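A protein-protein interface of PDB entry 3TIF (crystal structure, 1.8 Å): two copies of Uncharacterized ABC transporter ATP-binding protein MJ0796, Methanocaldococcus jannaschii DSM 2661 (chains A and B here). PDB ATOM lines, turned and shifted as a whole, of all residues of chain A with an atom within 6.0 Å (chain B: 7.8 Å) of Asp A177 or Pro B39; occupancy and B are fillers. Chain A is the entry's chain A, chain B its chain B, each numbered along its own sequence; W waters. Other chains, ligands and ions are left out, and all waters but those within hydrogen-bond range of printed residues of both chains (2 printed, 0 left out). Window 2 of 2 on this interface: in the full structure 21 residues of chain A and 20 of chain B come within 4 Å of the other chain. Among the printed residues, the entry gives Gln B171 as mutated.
OG of Ser B40 sits at hydrogen-bond distance from NH2 of Arg A153 (2.8 Å). N of Ser B40 is in hydrogen-bond range of OD1 of Asp A177, at 3.0 Å. The backbone carbonyl oxygen of Ala A175 is in hydrogen-bond range of a ring nitrogen (NE2) of His B204 (3.5 Å).
OG of Ser B42 is in hydrogen-bond range of O of Pro B39. The side-chain carboxylate (OD2) of Asp A177 is in hydrogen-bond range of the side-chain hydroxyl (OG1) of Thr A180. The backbone NH of Lys A179 lies close to the side-chain carboxylate of Asp A177, 3.5 Å away. The side-chain amino group of Lys B44 sits at hydrogen-bond distance from the backbone carbonyl oxygen of Pro B39 (3.0 Å).
Among the printed residues, merely in contact across the chains: Asp A177 with His B204 (3.4 Å), Asp A177 with Pro B39 (3.7 Å) and Leu A176 with His B204 (3.7 Å).
Printed residues of chain B within 4 Å of Asp A177: Pro B39, Ser B40 and His B204. Of chain A, only Asp A177 (3.7 Å) comes within 4 Å of Pro B39. Of the printed residues of chain A, Ser B40 touches Arg A153 (2.8 Å) and Asp A177 (3.0 Å). Of the printed residues of chain B, Leu A176 touches His B204. Of the printed residues of chain A, His B204 touches Ala A175 (3.5 Å), Leu A176 (3.7 Å) and Asp A177 (3.4 Å). Printed residues of chain B within 4 Å of Arg A153: Ser B40. The nearest residue of chain B that does not touch Asp A177 is Gly B38 (4.4 Å). The nearest residue of chain A that does not touch Pro B39 is Thr A180 (5.9 Å).
Of the 10 printed residues of chain A, 4 touch a printed residue of chain B. Printed residues of chain A that touch a printed residue of chain B: Arg A153, Ala A175, Leu A176 and Asp A177. Along chain A the printed residues that touch a printed residue of chain B span positions 153 to 177. Among the printed residues, 6 pairs touch across the chains.
No position is printed for both chains.
Water W1 bridges the backbone carbonyl oxygen of His B204 and the backbone NH of Ser A178. Water W2 lies within hydrogen-bond range of the side-chain hydroxyl of Ser A178 and the backbone carbonyl oxygen of His B204.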
ATOM      1  N   ARG A 153      18.090 -11.878 -33.019  1.00  0.00           N
ATOM      2  CA  ARG A 153      16.650 -11.823 -33.249  1.00  0.00           C
ATOM      3  C   ARG A 153      16.281 -11.853 -34.725  1.00  0.00           C
ATOM      4  O   ARG A 153      15.278 -12.448 -35.110  1.00  0.00           O
ATOM      5  CB  ARG A 153      16.044 -10.611 -32.523  1.00  0.00           C
ATOM      6  CG  ARG A 153      15.965 -10.874 -31.015  1.00  0.00           C
ATOM      7  CD  ARG A 153      15.605  -9.647 -30.213  1.00  0.00           C
ATOM      8  NE  ARG A 153      16.763  -8.797 -29.949  1.00  0.00           N
ATOM      9  CZ  ARG A 153      16.689  -7.584 -29.412  1.00  0.00           C
ATOM     10  NH1 ARG A 153      15.501  -7.077 -29.105  1.00  0.00           N
ATOM     11  NH2 ARG A 153      17.795  -6.877 -29.189  1.00  0.00           N
ATOM     12  N   THR A 173      19.511 -17.683 -27.285  1.00  0.00           N
ATOM     13  CA  THR A 173      19.402 -16.571 -26.331  1.00  0.00           C
ATOM     14  C   THR A 173      20.765 -16.050 -25.895  1.00  0.00           C
ATOM     15  O   THR A 173      20.849 -15.220 -24.992  1.00  0.00           O
ATOM     16  CB  THR A 173      18.657 -17.000 -25.038  1.00  0.00           C
ATOM     17  OG1 THR A 173      19.416 -18.010 -24.365  1.00  0.00           O
ATOM     18  CG2 THR A 173      17.285 -17.524 -25.362  1.00  0.00           C
ATOM     19  N   ALA A 175      23.031 -14.064 -26.904  1.00  0.00           N
ATOM     20  CA  ALA A 175      23.387 -12.654 -27.034  1.00  0.00           C
ATOM     21  C   ALA A 175      22.321 -11.741 -26.444  1.00  0.00           C
ATOM     22  O   ALA A 175      22.344 -10.519 -26.649  1.00  0.00           O
ATOM     23  CB  ALA A 175      23.642 -12.302 -28.519  1.00  0.00           C
ATOM     24  N   LEU A 176      21.385 -12.337 -25.710  1.00  0.00           N
ATOM     25  CA  LEU A 176      20.256 -11.597 -25.162  1.00  0.00           C
ATOM     26  C   LEU A 176      20.359 -11.480 -23.639  1.00  0.00           C
ATOM     27  O   LEU A 176      20.798 -12.403 -22.961  1.00  0.00           O
ATOM     28  CB  LEU A 176      18.937 -12.293 -25.538  1.00  0.00           C
ATOM     29  CG  LEU A 176      18.663 -12.498 -27.029  1.00  0.00           C
ATOM     30  CD1 LEU A 176      17.310 -13.159 -27.251  1.00  0.00           C
ATOM     31  CD2 LEU A 176      18.722 -11.167 -27.742  1.00  0.00           C
ATOM     32  N   ASP A 177      19.950 -10.331 -23.119  1.00  0.00           N
ATOM     33  CA  ASP A 177      19.809 -10.150 -21.689  1.00  0.00           C
ATOM     34  C   ASP A 177      18.682 -11.074 -21.223  1.00  0.00           C
ATOM     35  O   ASP A 177      17.892 -11.579 -22.031  1.00  0.00           O
ATOM     36  CB  ASP A 177      19.459  -8.693 -21.405  1.00  0.00           C
ATOM     37  CG  ASP A 177      18.281  -8.228 -22.218  1.00  0.00           C
ATOM     38  OD1 ASP A 177      18.471  -7.859 -23.404  1.00  0.00           O
ATOM     39  OD2 ASP A 177      17.159  -8.261 -21.688  1.00  0.00           O
ATOM     40  N   SER A 178      18.612 -11.297 -19.919  1.00  0.00           N
ATOM     41  CA  SER A 178      17.671 -12.263 -19.357  1.00  0.00           C
ATOM     42  C   SER A 178      16.218 -12.031 -19.758  1.00  0.00           C
ATOM     43  O   SER A 178      15.509 -12.977 -20.078  1.00  0.00           O
ATOM     44  CB  SER A 178      17.792 -12.278 -17.832  1.00  0.00           C
ATOM     45  OG  SER A 178      19.107 -12.636 -17.449  1.00  0.00           O
ATOM     46  N   LYS A 179      15.769 -10.782 -19.719  1.00  0.00           N
ATOM     47  CA  LYS A 179      14.359 -10.481 -19.982  1.00  0.00           C
ATOM     48  C   LYS A 179      13.960 -10.756 -21.425  1.00  0.00           C
ATOM     49  O   LYS A 179      12.888 -11.299 -21.693  1.00  0.00           O
ATOM     50  CB  LYS A 179      14.033  -9.025 -19.643  1.00  0.00           C
ATOM     51  CG  LYS A 179      14.115  -8.697 -18.164  1.00  0.00           C
ATOM     52  CD  LYS A 179      13.401  -7.383 -17.859  1.00  0.00           C
ATOM     53  CE  LYS A 179      13.715  -6.923 -16.449  1.00  0.00           C
ATOM     54  NZ  LYS A 179      13.906  -8.093 -15.555  1.00  0.00           N
ATOM     55  N   THR A 180      14.818 -10.347 -22.354  1.00  0.00           N
ATOM     56  CA  THR A 180      14.546 -10.529 -23.766  1.00  0.00           C
ATOM     57  C   THR A 180      14.635 -12.005 -24.142  1.00  0.00           C
ATOM     58  O   THR A 180      13.808 -12.512 -24.904  1.00  0.00           O
ATOM     59  CB  THR A 180      15.520  -9.720 -24.623  1.00  0.00           C
ATOM     60  OG1 THR A 180      15.435  -8.332 -24.250  1.00  0.00           O
ATOM     61  CG2 THR A 180      15.161  -9.881 -26.109  1.00  0.00           C
ATOM     62  N   GLY A 181      15.636 -12.690 -23.607  1.00  0.00           N
ATOM     63  CA  GLY A 181      15.764 -14.127 -23.799  1.00  0.00           C
ATOM     64  C   GLY A 181      14.540 -14.866 -23.289  1.00  0.00           C
ATOM     65  O   GLY A 181      14.087 -15.828 -23.894  1.00  0.00           O
ATOM     66  N   GLU A 182      13.989 -14.412 -22.171  1.00  0.00           N
ATOM     67  CA  GLU A 182      12.788 -15.051 -21.633  1.00  0.00           C
ATOM     68  C   GLU A 182      11.610 -14.917 -22.598  1.00  0.00           C
ATOM     69  O   GLU A 182      10.833 -15.851 -22.768  1.00  0.00           O
ATOM     70  CB  GLU A 182      12.423 -14.465 -20.269  1.00  0.00           C
ATOM     71  CG  GLU A 182      11.072 -14.946 -19.729  1.00  0.00           C
ATOM     72  CD  GLU A 182      11.117 -16.369 -19.208  1.00  0.00           C
ATOM     73  OE1 GLU A 182      12.233 -16.905 -19.031  1.00  0.00           O
ATOM     74  OE2 GLU A 182      10.032 -16.951 -18.972  1.00  0.00           O
ATOM     75  N   MET B  37      26.869  -4.274 -17.754  1.00  0.00           N
ATOM     76  CA  MET B  37      25.679  -5.033 -18.112  1.00  0.00           C
ATOM     77  C   MET B  37      24.642  -4.090 -18.667  1.00  0.00           C
ATOM     78  O   MET B  37      24.740  -2.875 -18.508  1.00  0.00           O
ATOM     79  CB  MET B  37      25.094  -5.729 -16.871  1.00  0.00           C
ATOM     80  CG  MET B  37      25.994  -6.771 -16.252  1.00  0.00           C
ATOM     81  SD  MET B  37      25.166  -7.673 -14.905  1.00  0.00           S
ATOM     82  CE  MET B  37      24.195  -8.845 -15.853  1.00  0.00           C
ATOM     83  N   GLY B  38      23.623  -4.645 -19.306  1.00  0.00           N
ATOM     84  CA  GLY B  38      22.558  -3.812 -19.836  1.00  0.00           C
ATOM     85  C   GLY B  38      21.860  -4.497 -20.990  1.00  0.00           C
ATOM     86  O   GLY B  38      22.399  -5.453 -21.577  1.00  0.00           O
ATOM     87  N   PRO B  39      20.666  -4.001 -21.351  1.00  0.00           N
ATOM     88  CA  PRO B  39      19.865  -4.618 -22.415  1.00  0.00           C
ATOM     89  C   PRO B  39      20.594  -4.704 -23.756  1.00  0.00           C
ATOM     90  O   PRO B  39      21.490  -3.906 -24.051  1.00  0.00           O
ATOM     91  CB  PRO B  39      18.650  -3.696 -22.519  1.00  0.00           C
ATOM     92  CG  PRO B  39      18.537  -3.079 -21.150  1.00  0.00           C
ATOM     93  CD  PRO B  39      19.963  -2.875 -20.708  1.00  0.00           C
ATOM     94  N   SER B  40      20.222  -5.701 -24.554  1.00  0.00           N
ATOM     95  CA  SER B  40      20.752  -5.824 -25.898  1.00  0.00           C
ATOM     96  C   SER B  40      20.590  -4.467 -26.568  1.00  0.00           C
ATOM     97  O   SER B  40      19.516  -3.869 -26.523  1.00  0.00           O
ATOM     98  CB  SER B  40      20.013  -6.937 -26.665  1.00  0.00           C
ATOM     99  OG  SER B  40      20.376  -6.972 -28.033  1.00  0.00           O
ATOM    100  N   GLY B  41      21.676  -3.952 -27.132  1.00  0.00           N
ATOM    101  CA  GLY B  41      21.643  -2.677 -27.822  1.00  0.00           C
ATOM    102  C   GLY B  41      21.795  -1.428 -26.973  1.00  0.00           C
ATOM    103  O   GLY B  41      21.609  -0.320 -27.481  1.00  0.00           O
ATOM    104  N   SER B  42      22.139  -1.583 -25.695  1.00  0.00           N
ATOM    105  CA  SER B  42      22.217  -0.436 -24.783  1.00  0.00           C
ATOM    106  C   SER B  42      23.522   0.371 -24.890  1.00  0.00           C
ATOM    107  O   SER B  42      23.643   1.439 -24.293  1.00  0.00           O
ATOM    108  CB  SER B  42      21.970  -0.864 -23.329  1.00  0.00           C
ATOM    109  OG  SER B  42      23.005  -1.709 -22.839  1.00  0.00           O
ATOM    110  N   GLY B  43      24.494  -0.139 -25.637  1.00  0.00           N
ATOM    111  CA  GLY B  43      25.729   0.596 -25.848  1.00  0.00           C
ATOM    112  C   GLY B  43      26.980  -0.012 -25.227  1.00  0.00           C
ATOM    113  O   GLY B  43      28.021   0.648 -25.149  1.00  0.00           O
ATOM    114  N   LYS B  44      26.899  -1.273 -24.808  1.00  0.00           N
ATOM    115  CA  LYS B  44      28.024  -1.930 -24.141  1.00  0.00           C
ATOM    116  C   LYS B  44      29.223  -2.156 -25.050  1.00  0.00           C
ATOM    117  O   LYS B  44      30.361  -1.827 -24.687  1.00  0.00           O
ATOM    118  CB  LYS B  44      27.571  -3.262 -23.517  1.00  0.00           C
ATOM    119  CG  LYS B  44      26.299  -3.118 -22.684  1.00  0.00           C
ATOM    120  CD  LYS B  44      25.806  -4.452 -22.090  1.00  0.00           C
ATOM    121  CE  LYS B  44      25.457  -5.477 -23.169  1.00  0.00           C
ATOM    122  NZ  LYS B  44      24.318  -5.033 -24.046  1.00  0.00           N
ATOM    123  N   GLN B 171      31.462 -10.312 -23.464  1.00  0.00           N
ATOM    124  CA  GLN B 171      30.711 -11.550 -23.274  1.00  0.00           C
ATOM    125  C   GLN B 171      31.614 -12.783 -23.411  1.00  0.00           C
ATOM    126  O   GLN B 171      31.334 -13.684 -24.200  1.00  0.00           O
ATOM    127  CB  GLN B 171      29.518 -11.576 -24.252  1.00  0.00           C
ATOM    128  CG  GLN B 171      28.713 -10.263 -24.188  1.00  0.00           C
ATOM    129  CD  GLN B 171      27.481 -10.238 -25.074  1.00  0.00           C
ATOM    130  OE1 GLN B 171      26.940 -11.274 -25.415  1.00  0.00           O
ATOM    131  NE2 GLN B 171      27.028  -9.034 -25.442  1.00  0.00           N
ATOM    132  N   THR B 203      28.837  -8.442 -19.953  1.00  0.00           N
ATOM    133  CA  THR B 203      28.190  -9.731 -19.749  1.00  0.00           C
ATOM    134  C   THR B 203      26.693  -9.581 -19.511  1.00  0.00           C
ATOM    135  O   THR B 203      26.217  -8.526 -19.057  1.00  0.00           O
ATOM    136  CB  THR B 203      28.830 -10.529 -18.569  1.00  0.00           C
ATOM    137  OG1 THR B 203      28.325 -11.873 -18.554  1.00  0.00           O
ATOM    138  CG2 THR B 203      28.496  -9.873 -17.238  1.00  0.00           C
ATOM    139  N   HIS B 204      25.964 -10.632 -19.887  1.00  0.00           N
ATOM    140  CA  HIS B 204      24.551 -10.779 -19.587  1.00  0.00           C
ATOM    141  C   HIS B 204      24.374 -11.774 -18.430  1.00  0.00           C
ATOM    142  O   HIS B 204      23.255 -12.024 -18.000  1.00  0.00           O
ATOM    143  CB  HIS B 204      23.778 -11.282 -20.817  1.00  0.00           C
ATOM    144  CG  HIS B 204      23.593 -10.242 -21.878  1.00  0.00           C
ATOM    145  ND1 HIS B 204      23.014  -9.017 -21.629  1.00  0.00           N
ATOM    146  CD2 HIS B 204      23.885 -10.254 -23.204  1.00  0.00           C
ATOM    147  CE1 HIS B 204      22.969  -8.311 -22.746  1.00  0.00           C
ATOM    148  NE2 HIS B 204      23.497  -9.045 -23.717  1.00  0.00           N
ATOM    149  N   ASP B 205      25.481 -12.340 -17.952  1.00  0.00           N
ATOM    150  CA  ASP B 205      25.461 -13.356 -16.884  1.00  0.00           C
ATOM    151  C   ASP B 205      25.825 -12.709 -15.532  1.00  0.00           C
ATOM    152  O   ASP B 205      26.975 -12.328 -15.311  1.00  0.00           O
ATOM    153  CB  ASP B 205      26.439 -14.486 -17.247  1.00  0.00           C
ATOM    154  CG  ASP B 205      26.409 -15.652 -16.259  1.00  0.00           C
ATOM    155  OD1 ASP B 205      25.960 -15.472 -15.104  1.00  0.00           O
ATOM    156  OD2 ASP B 205      26.862 -16.751 -16.651  1.00  0.00           O
ATOM    157  N   TYR B 217      25.705  -0.391 -15.084  1.00  0.00           N
ATOM    158  CA  TYR B 217      24.533  -0.719 -15.882  1.00  0.00           C
ATOM    159  C   TYR B 217      24.237   0.350 -16.934  1.00  0.00           C
ATOM    160  O   TYR B 217      24.139   1.531 -16.606  1.00  0.00           O
ATOM    161  CB  TYR B 217      23.316  -0.916 -14.973  1.00  0.00           C
ATOM    162  CG  TYR B 217      23.422  -2.132 -14.090  1.00  0.00           C
ATOM    163  CD1 TYR B 217      24.035  -2.061 -12.844  1.00  0.00           C
ATOM    164  CD2 TYR B 217      22.916  -3.359 -14.503  1.00  0.00           C
ATOM    165  CE1 TYR B 217      24.133  -3.180 -12.033  1.00  0.00           C
ATOM    166  CE2 TYR B 217      23.012  -4.478 -13.699  1.00  0.00           C
ATOM    167  CZ  TYR B 217      23.622  -4.383 -12.471  1.00  0.00           C
ATOM    168  OH  TYR B 217      23.721  -5.506 -11.677  1.00  0.00           O
ATOM    169  N   LEU B 218      24.094  -0.073 -18.193  1.00  0.00           N
ATOM    170  CA  LEU B 218      23.778   0.846 -19.284  1.00  0.00           C
ATOM    171  C   LEU B 218      22.318   0.699 -19.695  1.00  0.00           C
ATOM    172  O   LEU B 218      21.721  -0.368 -19.548  1.00  0.00           O
ATOM    173  CB  LEU B 218      24.672   0.592 -20.513  1.00  0.00           C
ATOM    174  CG  LEU B 218      26.189   0.765 -20.367  1.00  0.00           C
ATOM    175  CD1 LEU B 218      26.879   0.671 -21.732  1.00  0.00           C
ATOM    176  CD2 LEU B 218      26.539   2.089 -19.674  1.00  0.00           C
ATOM    177  N   LYS B 219      21.757   1.777 -20.226  1.00  0.00           N
ATOM    178  CA  LYS B 219      20.385   1.784 -20.705  1.00  0.00           C
ATOM    179  C   LYS B 219      20.235   2.918 -21.707  1.00  0.00           C
ATOM    180  O   LYS B 219      20.535   4.062 -21.393  1.00  0.00           O
ATOM    181  CB  LYS B 219      19.417   2.002 -19.541  1.00  0.00           C
ATOM    182  CG  LYS B 219      17.954   2.121 -19.960  1.00  0.00           C
ATOM    183  CD  LYS B 219      17.056   2.350 -18.751  1.00  0.00           C
ATOM    184  CE  LYS B 219      15.589   2.418 -19.154  1.00  0.00           C
ATOM    185  NZ  LYS B 219      14.701   2.629 -17.980  1.00  0.00           N
ATOM    186  N   ASP B 220      19.791   2.596 -22.918  1.00  0.00           N
ATOM    187  CA  ASP B 220      19.588   3.625 -23.940  1.00  0.00           C
ATOM    188  C   ASP B 220      20.819   4.503 -24.156  1.00  0.00           C
ATOM    189  O   ASP B 220      20.692   5.702 -24.394  1.00  0.00           O
ATOM    190  CB  ASP B 220      18.397   4.512 -23.569  1.00  0.00           C
ATOM    191  CG  ASP B 220      17.077   3.768 -23.621  1.00  0.00           C
ATOM    192  OD1 ASP B 220      16.916   2.913 -24.518  1.00  0.00           O
ATOM    193  OD2 ASP B 220      16.203   4.037 -22.767  1.00  0.00           O
ATOM    194  N   GLU B 224      22.893   4.008 -16.496  1.00  0.00           N
ATOM    195  CA  GLU B 224      21.680   3.972 -15.692  1.00  0.00           C
ATOM    196  C   GLU B 224      22.024   3.993 -14.208  1.00  0.00           C
ATOM    197  O   GLU B 224      21.464   4.774 -13.439  1.00  0.00           O
ATOM    198  CB  GLU B 224      20.859   2.724 -16.012  1.00  0.00           C
ATOM    199  CG  GLU B 224      19.554   2.655 -15.232  1.00  0.00           C
ATOM    200  CD  GLU B 224      18.855   1.319 -15.361  1.00  0.00           C
ATOM    201  OE1 GLU B 224      19.473   0.359 -15.881  1.00  0.00           O
ATOM    202  OE2 GLU B 224      17.683   1.229 -14.939  1.00  0.00           O
HETATM  203  O   HOH W   1      20.865 -10.367 -18.222  1.00  0.00           O
HETATM  204  O   HOH W   2      21.024 -14.191 -19.068  1.00  0.00           O
